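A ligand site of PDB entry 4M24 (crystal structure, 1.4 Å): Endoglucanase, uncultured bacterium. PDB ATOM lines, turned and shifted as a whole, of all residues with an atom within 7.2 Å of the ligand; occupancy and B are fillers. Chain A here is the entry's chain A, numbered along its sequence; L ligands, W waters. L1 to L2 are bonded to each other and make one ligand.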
ATOM      1  N   HIS A  90      -3.742  10.504  -4.772  1.00  0.00           N
ATOM      2  CA  HIS A  90      -2.437  11.176  -4.690  1.00  0.00           C
ATOM      3  C   HIS A  90      -1.321  10.155  -4.608  1.00  0.00           C
ATOM      4  O   HIS A  90      -0.624  10.071  -3.595  1.00  0.00           O
ATOM      5  CB  HIS A  90      -2.441  12.104  -3.469  1.00  0.00           C
ATOM      6  CG  HIS A  90      -1.454  13.222  -3.536  1.00  0.00           C
ATOM      7  ND1 HIS A  90      -1.727  14.412  -4.177  1.00  0.00           N
ATOM      8  CD2 HIS A  90      -0.205  13.356  -3.022  1.00  0.00           C
ATOM      9  CE1 HIS A  90      -0.694  15.232  -4.043  1.00  0.00           C
ATOM     10  NE2 HIS A  90       0.234  14.607  -3.349  1.00  0.00           N
ATOM     11  N   TYR A  92       1.108   8.877  -7.430  1.00  0.00           N
ATOM     12  CA  TYR A  92       2.319   8.773  -8.244  1.00  0.00           C
ATOM     13  C   TYR A  92       2.305   7.526  -9.139  1.00  0.00           C
ATOM     14  O   TYR A  92       3.353   6.984  -9.478  1.00  0.00           O
ATOM     15  CB  TYR A  92       3.576   8.817  -7.349  1.00  0.00           C
ATOM     16  CG  TYR A  92       3.551   9.978  -6.388  1.00  0.00           C
ATOM     17  CD1 TYR A  92       3.985  11.240  -6.765  1.00  0.00           C
ATOM     18  CD2 TYR A  92       3.044   9.825  -5.093  1.00  0.00           C
ATOM     19  CE1 TYR A  92       3.940  12.316  -5.886  1.00  0.00           C
ATOM     20  CE2 TYR A  92       2.986  10.892  -4.205  1.00  0.00           C
ATOM     21  CZ  TYR A  92       3.440  12.141  -4.601  1.00  0.00           C
ATOM     22  OH  TYR A  92       3.372  13.200  -3.734  1.00  0.00           O
ATOM     23  N   ASN A 134      -2.205  11.629  -9.071  1.00  0.00           N
ATOM     24  CA  ASN A 134      -1.193  12.655  -8.867  1.00  0.00           C
ATOM     25  C   ASN A 134       0.189  12.219  -9.341  1.00  0.00           C
ATOM     26  O   ASN A 134       0.665  11.152  -8.965  1.00  0.00           O
ATOM     27  CB  ASN A 134      -1.090  12.979  -7.372  1.00  0.00           C
ATOM     28  CG  ASN A 134      -0.140  14.137  -7.101  1.00  0.00           C
ATOM     29  OD1 ASN A 134      -0.398  15.268  -7.521  1.00  0.00           O
ATOM     30  ND2 ASN A 134       0.952  13.858  -6.402  1.00  0.00           N
ATOM     31  N   GLU A 135       0.805  13.054 -10.180  1.00  0.00           N
ATOM     32  CA  GLU A 135       2.237  12.961 -10.507  1.00  0.00           C
ATOM     33  C   GLU A 135       2.827  11.574 -10.798  1.00  0.00           C
ATOM     34  O   GLU A 135       3.713  11.118 -10.095  1.00  0.00           O
ATOM     35  CB  GLU A 135       3.071  13.675  -9.437  1.00  0.00           C
ATOM     36  CG  GLU A 135       2.816  15.171  -9.421  1.00  0.00           C
ATOM     37  CD  GLU A 135       3.717  15.926  -8.476  1.00  0.00           C
ATOM     38  OE1 GLU A 135       4.623  15.316  -7.844  1.00  0.00           O
ATOM     39  OE2 GLU A 135       3.519  17.157  -8.349  1.00  0.00           O
ATOM     40  N   TYR A 137       5.553   9.402 -12.303  1.00  0.00           N
ATOM     41  CA  TYR A 137       6.956   9.759 -12.537  1.00  0.00           C
ATOM     42  C   TYR A 137       7.821   8.513 -12.636  1.00  0.00           C
ATOM     43  O   TYR A 137       7.428   7.445 -12.203  1.00  0.00           O
ATOM     44  CB  TYR A 137       7.505  10.664 -11.416  1.00  0.00           C
ATOM     45  CG  TYR A 137       7.805   9.953 -10.117  1.00  0.00           C
ATOM     46  CD1 TYR A 137       9.036   9.345  -9.912  1.00  0.00           C
ATOM     47  CD2 TYR A 137       6.866   9.892  -9.103  1.00  0.00           C
ATOM     48  CE1 TYR A 137       9.313   8.682  -8.734  1.00  0.00           C
ATOM     49  CE2 TYR A 137       7.143   9.238  -7.916  1.00  0.00           C
ATOM     50  CZ  TYR A 137       8.369   8.643  -7.741  1.00  0.00           C
ATOM     51  OH  TYR A 137       8.647   7.989  -6.564  1.00  0.00           O
ATOM     52  N   SER A 170       6.350  12.475 -15.675  1.00  0.00           N
ATOM     53  CA  SER A 170       7.397  13.356 -15.179  1.00  0.00           C
ATOM     54  C   SER A 170       6.826  14.379 -14.198  1.00  0.00           C
ATOM     55  O   SER A 170       7.013  15.599 -14.354  1.00  0.00           O
ATOM     56  CB  SER A 170       8.112  14.039 -16.353  1.00  0.00           C
ATOM     57  OG  SER A 170       9.350  14.635 -15.956  1.00  0.00           O
ATOM     58  N   TRP A 171       6.123  13.861 -13.192  1.00  0.00           N
ATOM     59  CA  TRP A 171       5.471  14.674 -12.169  1.00  0.00           C
ATOM     60  C   TRP A 171       4.504  15.700 -12.762  1.00  0.00           C
ATOM     61  O   TRP A 171       4.302  16.790 -12.215  1.00  0.00           O
ATOM     62  CB  TRP A 171       6.495  15.367 -11.255  1.00  0.00           C
ATOM     63  CG  TRP A 171       7.417  14.427 -10.525  1.00  0.00           C
ATOM     64  CD1 TRP A 171       7.178  13.793  -9.335  1.00  0.00           C
ATOM     65  CD2 TRP A 171       8.718  14.015 -10.954  1.00  0.00           C
ATOM     66  NE1 TRP A 171       8.267  13.015  -8.991  1.00  0.00           N
ATOM     67  CE2 TRP A 171       9.223  13.132  -9.963  1.00  0.00           C
ATOM     68  CE3 TRP A 171       9.511  14.306 -12.057  1.00  0.00           C
ATOM     69  CZ2 TRP A 171      10.481  12.548 -10.067  1.00  0.00           C
ATOM     70  CZ3 TRP A 171      10.769  13.722 -12.160  1.00  0.00           C
ATOM     71  CH2 TRP A 171      11.244  12.844 -11.171  1.00  0.00           C
ATOM     72  N   SER A 172       3.874  15.318 -13.865  1.00  0.00           N
ATOM     73  CA  SER A 172       2.950  16.187 -14.596  1.00  0.00           C
ATOM     74  C   SER A 172       3.558  17.549 -14.870  1.00  0.00           C
ATOM     75  O   SER A 172       2.863  18.574 -14.851  1.00  0.00           O
ATOM     76  CB  SER A 172       1.610  16.325 -13.871  1.00  0.00           C
ATOM     77  OG  SER A 172       0.587  16.486 -14.827  1.00  0.00           O
ATOM     78  N   SER A 173       4.856  17.571 -15.165  1.00  0.00           N
ATOM     79  CA  SER A 173       5.561  18.822 -15.373  1.00  0.00           C
ATOM     80  C   SER A 173       4.951  19.625 -16.513  1.00  0.00           C
ATOM     81  O   SER A 173       4.866  19.148 -17.657  1.00  0.00           O
ATOM     82  CB  SER A 173       7.031  18.541 -15.699  1.00  0.00           C
ATOM     83  OG  SER A 173       7.669  19.689 -16.213  1.00  0.00           O
ATOM     84  N   ARG A 176       8.021  20.533 -19.037  1.00  0.00           N
ATOM     85  CA  ARG A 176       8.474  19.499 -19.956  1.00  0.00           C
ATOM     86  C   ARG A 176       7.330  18.833 -20.698  1.00  0.00           C
ATOM     87  O   ARG A 176       7.540  17.846 -21.393  1.00  0.00           O
ATOM     88  CB  ARG A 176       9.202  18.418 -19.160  1.00  0.00           C
ATOM     89  CG  ARG A 176      10.478  18.880 -18.481  1.00  0.00           C
ATOM     90  CD  ARG A 176      11.216  17.750 -17.806  1.00  0.00           C
ATOM     91  NE  ARG A 176      10.494  17.181 -16.661  1.00  0.00           N
ATOM     92  CZ  ARG A 176      10.463  17.728 -15.444  1.00  0.00           C
ATOM     93  NH1 ARG A 176      11.095  18.861 -15.207  1.00  0.00           N
ATOM     94  NH2 ARG A 176       9.799  17.133 -14.476  1.00  0.00           N
ATOM     95  N   HIS A 199       1.532  20.522 -13.336  1.00  0.00           N
ATOM     96  CA  HIS A 199       2.015  21.110 -12.092  1.00  0.00           C
ATOM     97  C   HIS A 199       3.203  22.004 -12.378  1.00  0.00           C
ATOM     98  O   HIS A 199       3.991  21.723 -13.275  1.00  0.00           O
ATOM     99  CB  HIS A 199       2.421  20.011 -11.100  1.00  0.00           C
ATOM    100  CG  HIS A 199       1.274  19.196 -10.600  1.00  0.00           C
ATOM    101  ND1 HIS A 199       1.427  18.204  -9.656  1.00  0.00           N
ATOM    102  CD2 HIS A 199      -0.042  19.231 -10.907  1.00  0.00           C
ATOM    103  CE1 HIS A 199       0.251  17.643  -9.416  1.00  0.00           C
ATOM    104  NE2 HIS A 199      -0.657  18.246 -10.169  1.00  0.00           N
ATOM    105  N   VAL A 200       3.321  23.084 -11.637  1.00  0.00           N
ATOM    106  CA  VAL A 200       4.426  24.011 -11.828  1.00  0.00           C
ATOM    107  C   VAL A 200       4.869  24.635 -10.506  1.00  0.00           C
ATOM    108  O   VAL A 200       4.076  25.225  -9.767  1.00  0.00           O
ATOM    109  CB  VAL A 200       4.084  25.110 -12.866  1.00  0.00           C
ATOM    110  CG1 VAL A 200       2.786  25.797 -12.513  1.00  0.00           C
ATOM    111  CG2 VAL A 200       5.219  26.121 -12.983  1.00  0.00           C
ATOM    112  N   TYR A 201       6.165  24.482 -10.212  1.00  0.00           N
ATOM    113  CA  TYR A 201       6.819  25.216  -9.144  1.00  0.00           C
ATOM    114  C   TYR A 201       7.943  26.018  -9.776  1.00  0.00           C
ATOM    115  O   TYR A 201       8.496  25.618 -10.802  1.00  0.00           O
ATOM    116  CB  TYR A 201       7.355  24.245  -8.091  1.00  0.00           C
ATOM    117  CG  TYR A 201       6.233  23.553  -7.358  1.00  0.00           C
ATOM    118  CD1 TYR A 201       5.617  24.145  -6.254  1.00  0.00           C
ATOM    119  CD2 TYR A 201       5.752  22.327  -7.796  1.00  0.00           C
ATOM    120  CE1 TYR A 201       4.566  23.533  -5.605  1.00  0.00           C
ATOM    121  CE2 TYR A 201       4.697  21.696  -7.147  1.00  0.00           C
ATOM    122  CZ  TYR A 201       4.115  22.302  -6.051  1.00  0.00           C
ATOM    123  OH  TYR A 201       3.073  21.689  -5.391  1.00  0.00           O
ATOM    124  N   ASP A 203      10.876  27.205  -8.256  1.00  0.00           N
ATOM    125  CA  ASP A 203      12.237  27.036  -7.777  1.00  0.00           C
ATOM    126  C   ASP A 203      13.097  26.442  -8.893  1.00  0.00           C
ATOM    127  O   ASP A 203      12.577  26.070  -9.947  1.00  0.00           O
ATOM    128  CB  ASP A 203      12.312  26.202  -6.486  1.00  0.00           C
ATOM    129  CG  ASP A 203      11.640  24.840  -6.598  1.00  0.00           C
ATOM    130  OD1 ASP A 203      10.817  24.598  -7.503  1.00  0.00           O
ATOM    131  OD2 ASP A 203      11.926  23.998  -5.712  1.00  0.00           O
ATOM    132  N   GLU A 204      14.402  26.361  -8.687  1.00  0.00           N
ATOM    133  CA  GLU A 204      15.269  25.989  -9.780  1.00  0.00           C
ATOM    134  C   GLU A 204      14.979  24.621 -10.396  1.00  0.00           C
ATOM    135  O   GLU A 204      14.906  24.519 -11.616  1.00  0.00           O
ATOM    136  CB  GLU A 204      16.720  26.047  -9.272  1.00  0.00           C
ATOM    137  CG  GLU A 204      17.775  25.834 -10.320  1.00  0.00           C
ATOM    138  CD  GLU A 204      19.172  25.920  -9.715  1.00  0.00           C
ATOM    139  OE1 GLU A 204      19.315  26.531  -8.636  1.00  0.00           O
ATOM    140  OE2 GLU A 204      20.093  25.355 -10.325  1.00  0.00           O
ATOM    141  N   ASP A 205      14.762  23.616  -9.579  1.00  0.00           N
ATOM    142  CA  ASP A 205      14.491  22.274 -10.103  1.00  0.00           C
ATOM    143  C   ASP A 205      12.996  21.940 -10.246  1.00  0.00           C
ATOM    144  O   ASP A 205      12.636  20.813 -10.573  1.00  0.00           O
ATOM    145  CB  ASP A 205      15.208  21.205  -9.268  1.00  0.00           C
ATOM    146  CG  ASP A 205      14.596  21.007  -7.891  1.00  0.00           C
ATOM    147  OD1 ASP A 205      13.697  21.777  -7.508  1.00  0.00           O
ATOM    148  OD2 ASP A 205      15.042  20.080  -7.175  1.00  0.00           O
ATOM    149  N   ALA A 206      12.135  22.929  -9.989  1.00  0.00           N
ATOM    150  CA  ALA A 206      10.690  22.770 -10.116  1.00  0.00           C
ATOM    151  C   ALA A 206      10.098  21.696  -9.197  1.00  0.00           C
ATOM    152  O   ALA A 206       9.015  21.171  -9.452  1.00  0.00           O
ATOM    153  CB  ALA A 206      10.292  22.517 -11.582  1.00  0.00           C
ATOM    154  N   SER A 207      10.821  21.382  -8.134  1.00  0.00           N
ATOM    155  CA  SER A 207      10.371  20.384  -7.164  1.00  0.00           C
ATOM    156  C   SER A 207       9.474  20.985  -6.091  1.00  0.00           C
ATOM    157  O   SER A 207       8.792  20.246  -5.366  1.00  0.00           O
ATOM    158  CB  SER A 207      11.568  19.721  -6.471  1.00  0.00           C
ATOM    159  OG  SER A 207      12.209  20.645  -5.603  1.00  0.00           O
ATOM    160  N   GLY A 208       9.476  22.302  -5.978  1.00  0.00           N
ATOM    161  CA  GLY A 208       8.760  22.952  -4.892  1.00  0.00           C
ATOM    162  C   GLY A 208       9.454  22.932  -3.547  1.00  0.00           C
ATOM    163  O   GLY A 208       8.860  23.370  -2.564  1.00  0.00           O
ATOM    164  N   SER A 209      10.696  22.448  -3.471  1.00  0.00           N
ATOM    165  CA  SER A 209      11.414  22.476  -2.195  1.00  0.00           C
ATOM    166  C   SER A 209      11.993  23.860  -1.878  1.00  0.00           C
ATOM    167  O   SER A 209      12.299  24.157  -0.730  1.00  0.00           O
ATOM    168  CB  SER A 209      12.502  21.400  -2.135  1.00  0.00           C
ATOM    169  OG  SER A 209      13.452  21.571  -3.176  1.00  0.00           O
ATOM    170  N   ARG A 226       7.217  28.558 -17.778  1.00  0.00           N
ATOM    171  CA  ARG A 226       7.138  27.143 -17.476  1.00  0.00           C
ATOM    172  C   ARG A 226       5.799  26.513 -17.831  1.00  0.00           C
ATOM    173  O   ARG A 226       5.732  25.310 -18.027  1.00  0.00           O
ATOM    174  CB  ARG A 226       7.524  26.860 -16.036  1.00  0.00           C
ATOM    175  CG  ARG A 226       9.025  26.958 -15.855  1.00  0.00           C
ATOM    176  CD  ARG A 226       9.461  26.526 -14.483  1.00  0.00           C
ATOM    177  NE  ARG A 226      10.909  26.583 -14.376  1.00  0.00           N
ATOM    178  CZ  ARG A 226      11.579  26.329 -13.267  1.00  0.00           C
ATOM    179  NH1 ARG A 226      10.922  26.004 -12.165  1.00  0.00           N
ATOM    180  NH2 ARG A 226      12.897  26.422 -13.249  1.00  0.00           N
ATOM    181  N   GLU A 245      -1.269  22.121  -9.225  1.00  0.00           N
ATOM    182  CA  GLU A 245      -0.383  22.561  -8.133  1.00  0.00           C
ATOM    183  C   GLU A 245       0.530  23.680  -8.587  1.00  0.00           C
ATOM    184  O   GLU A 245       1.133  23.607  -9.657  1.00  0.00           O
ATOM    185  CB  GLU A 245       0.499  21.420  -7.638  1.00  0.00           C
ATOM    186  CG  GLU A 245      -0.250  20.258  -7.032  1.00  0.00           C
ATOM    187  CD  GLU A 245       0.658  19.201  -6.414  1.00  0.00           C
ATOM    188  OE1 GLU A 245       1.866  19.482  -6.232  1.00  0.00           O
ATOM    189  OE2 GLU A 245       0.174  18.101  -6.078  1.00  0.00           O
HETATM  190  C1  LIG L   1      11.872  17.719 -11.551  1.00  0.00           C
HETATM  191  C2  LIG L   1      11.183  17.769 -10.197  1.00  0.00           C
HETATM  192  C3  LIG L   1      11.458  16.485  -9.407  1.00  0.00           C
HETATM  193  C4  LIG L   1      12.952  16.191  -9.380  1.00  0.00           C
HETATM  194  C5  LIG L   1      13.236  14.846  -8.720  1.00  0.00           C
HETATM  195  C6  LIG L   1      13.348  17.464 -11.324  1.00  0.00           C
HETATM  196  O1  LIG L   1      13.993  17.430 -12.591  1.00  0.00           O
HETATM  197  O2  LIG L   1      11.664  18.950 -12.277  1.00  0.00           O
HETATM  198  O3  LIG L   1       9.772  17.931 -10.419  1.00  0.00           O
HETATM  199  O4  LIG L   1      11.037  16.610  -8.043  1.00  0.00           O
HETATM  200  O5  LIG L   1      13.474  16.189 -10.695  1.00  0.00           O
HETATM  201  O6  LIG L   1      14.644  14.627  -8.599  1.00  0.00           O
HETATM  202  C1  LG2 L   2       9.602  15.818  -6.330  1.00  0.00           C
HETATM  203  C2  LG2 L   2       8.153  15.557  -5.938  1.00  0.00           C
HETATM  204  C3  LG2 L   2       7.316  16.807  -6.218  1.00  0.00           C
HETATM  205  C4  LG2 L   2       7.512  17.272  -7.653  1.00  0.00           C
HETATM  206  C5  LG2 L   2       6.830  18.615  -7.881  1.00  0.00           C
HETATM  207  C6  LG2 L   2       9.688  16.292  -7.774  1.00  0.00           C
HETATM  208  O1  LG2 L   2      10.368  14.634  -6.165  1.00  0.00           O
HETATM  209  O2  LG2 L   2       8.080  15.244  -4.552  1.00  0.00           O
HETATM  210  O3  LG2 L   2       5.951  16.503  -5.960  1.00  0.00           O
HETATM  211  O4  LG2 L   2       8.898  17.470  -7.901  1.00  0.00           O
HETATM  212  O5  LG2 L   2       7.141  19.088  -9.208  1.00  0.00           O
HETATM  213  O   HOH W   1       6.840  21.779 -11.411  1.00  0.00           O
HETATM  214  O   HOH W   2       5.975  18.972 -11.691  1.00  0.00           O
HETATM  215  O   HOH W   3      13.031  15.859 -14.712  1.00  0.00           O
HETATM  216  O   HOH W   4      16.639  17.279 -12.107  1.00  0.00           O
HETATM  217  O   HOH W   5       9.461  12.028  -6.496  1.00  0.00           O
HETATM  218  O   HOH W   6       8.568  19.086 -12.643  1.00  0.00           O
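CH2 of Trp 171 touches C5 of LIG L1, at 3.7 Å.
Tyr 201 touches the ligand.
CA of Ser 207 touches O4 of LG2 L2 (3.3 Å).
Hydrophobic or aromatic side chains that line the ligand: Trp 171, Tyr 201 and Ala 206.
The nearest printed residue that does not touch the ligand is Tyr 92 (4.6 Å).
The side-chain hydroxyl (OH) of Tyr 201 is in hydrogen-bond range of the side-chain carboxylate (OE1) of Glu 245 (2.7 Å).
The side-chain hydroxyl (OG) of Ser 170 is in hydrogen-bond range of the guanidinium group (NE) of Arg 176 (2.9 Å).
N of Ser 207 is in hydrogen-bond range of OD1 of Asp 203 (3.3 Å).
The backbone NH (N) of Ala 206 sits close to the side-chain carboxylate (OD1) of Asp 203 (3.3 Å).
ND1 of His 199 is in hydrogen-bond range of OE2 of Glu 135 (2.7 Å).
The side-chain hydroxyl (OG) of Ser 173 sits at hydrogen-bond distance from the backbone NH (N) of Arg 176, 3.0 Å away.
The side-chain hydroxyl of Ser 209 is in hydrogen-bond range of the side-chain hydroxyl of Ser 207.
OG of Ser 207 sits at hydrogen-bond distance from OD1 of Asp 205.
The side-chain carboxylate (OE1) of Glu 135 lies within hydrogen-bond range of an oxygen (O3) of LG2 L2 (2.6 Å).
NH1 of Arg 176 lies within hydrogen-bond range of O2 of LIG L1, 3.0 Å away.
O2 of LIG L1 sits at hydrogen-bond distance from O of Asp 205 (2.7 Å).
O5 of LG2 L2 lies within hydrogen-bond range of O of Ala 206, at 2.8 Å.
Water W2 bridges O5 of LG2 L2 (2.7 Å) and O of Trp 171 (2.8 Å).
Water W5 bridges an oxygen (O1) of LG2 L2 (2.8 Å) and the indole nitrogen (NE1) of Trp 171 (2.9 Å).
Water W6 lies within hydrogen-bond range of O3 of LIG L1 (2.8 Å) and NH2 of Arg 176 (2.9 Å).
Water W3 lies within hydrogen-bond range of O1 of LIG L1 (2.8 Å) and NE of Arg 176 (3.5 Å).
Water W1 lies within hydrogen-bond range of the backbone carbonyl oxygen (O) of Ala 206 (3.0 Å), the backbone NH (N) of Tyr 201 (3.0 Å), the backbone carbonyl oxygen (O) of His 199 (3.4 Å) and an oxygen (O5) of LG2 L2 (3.5 Å).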
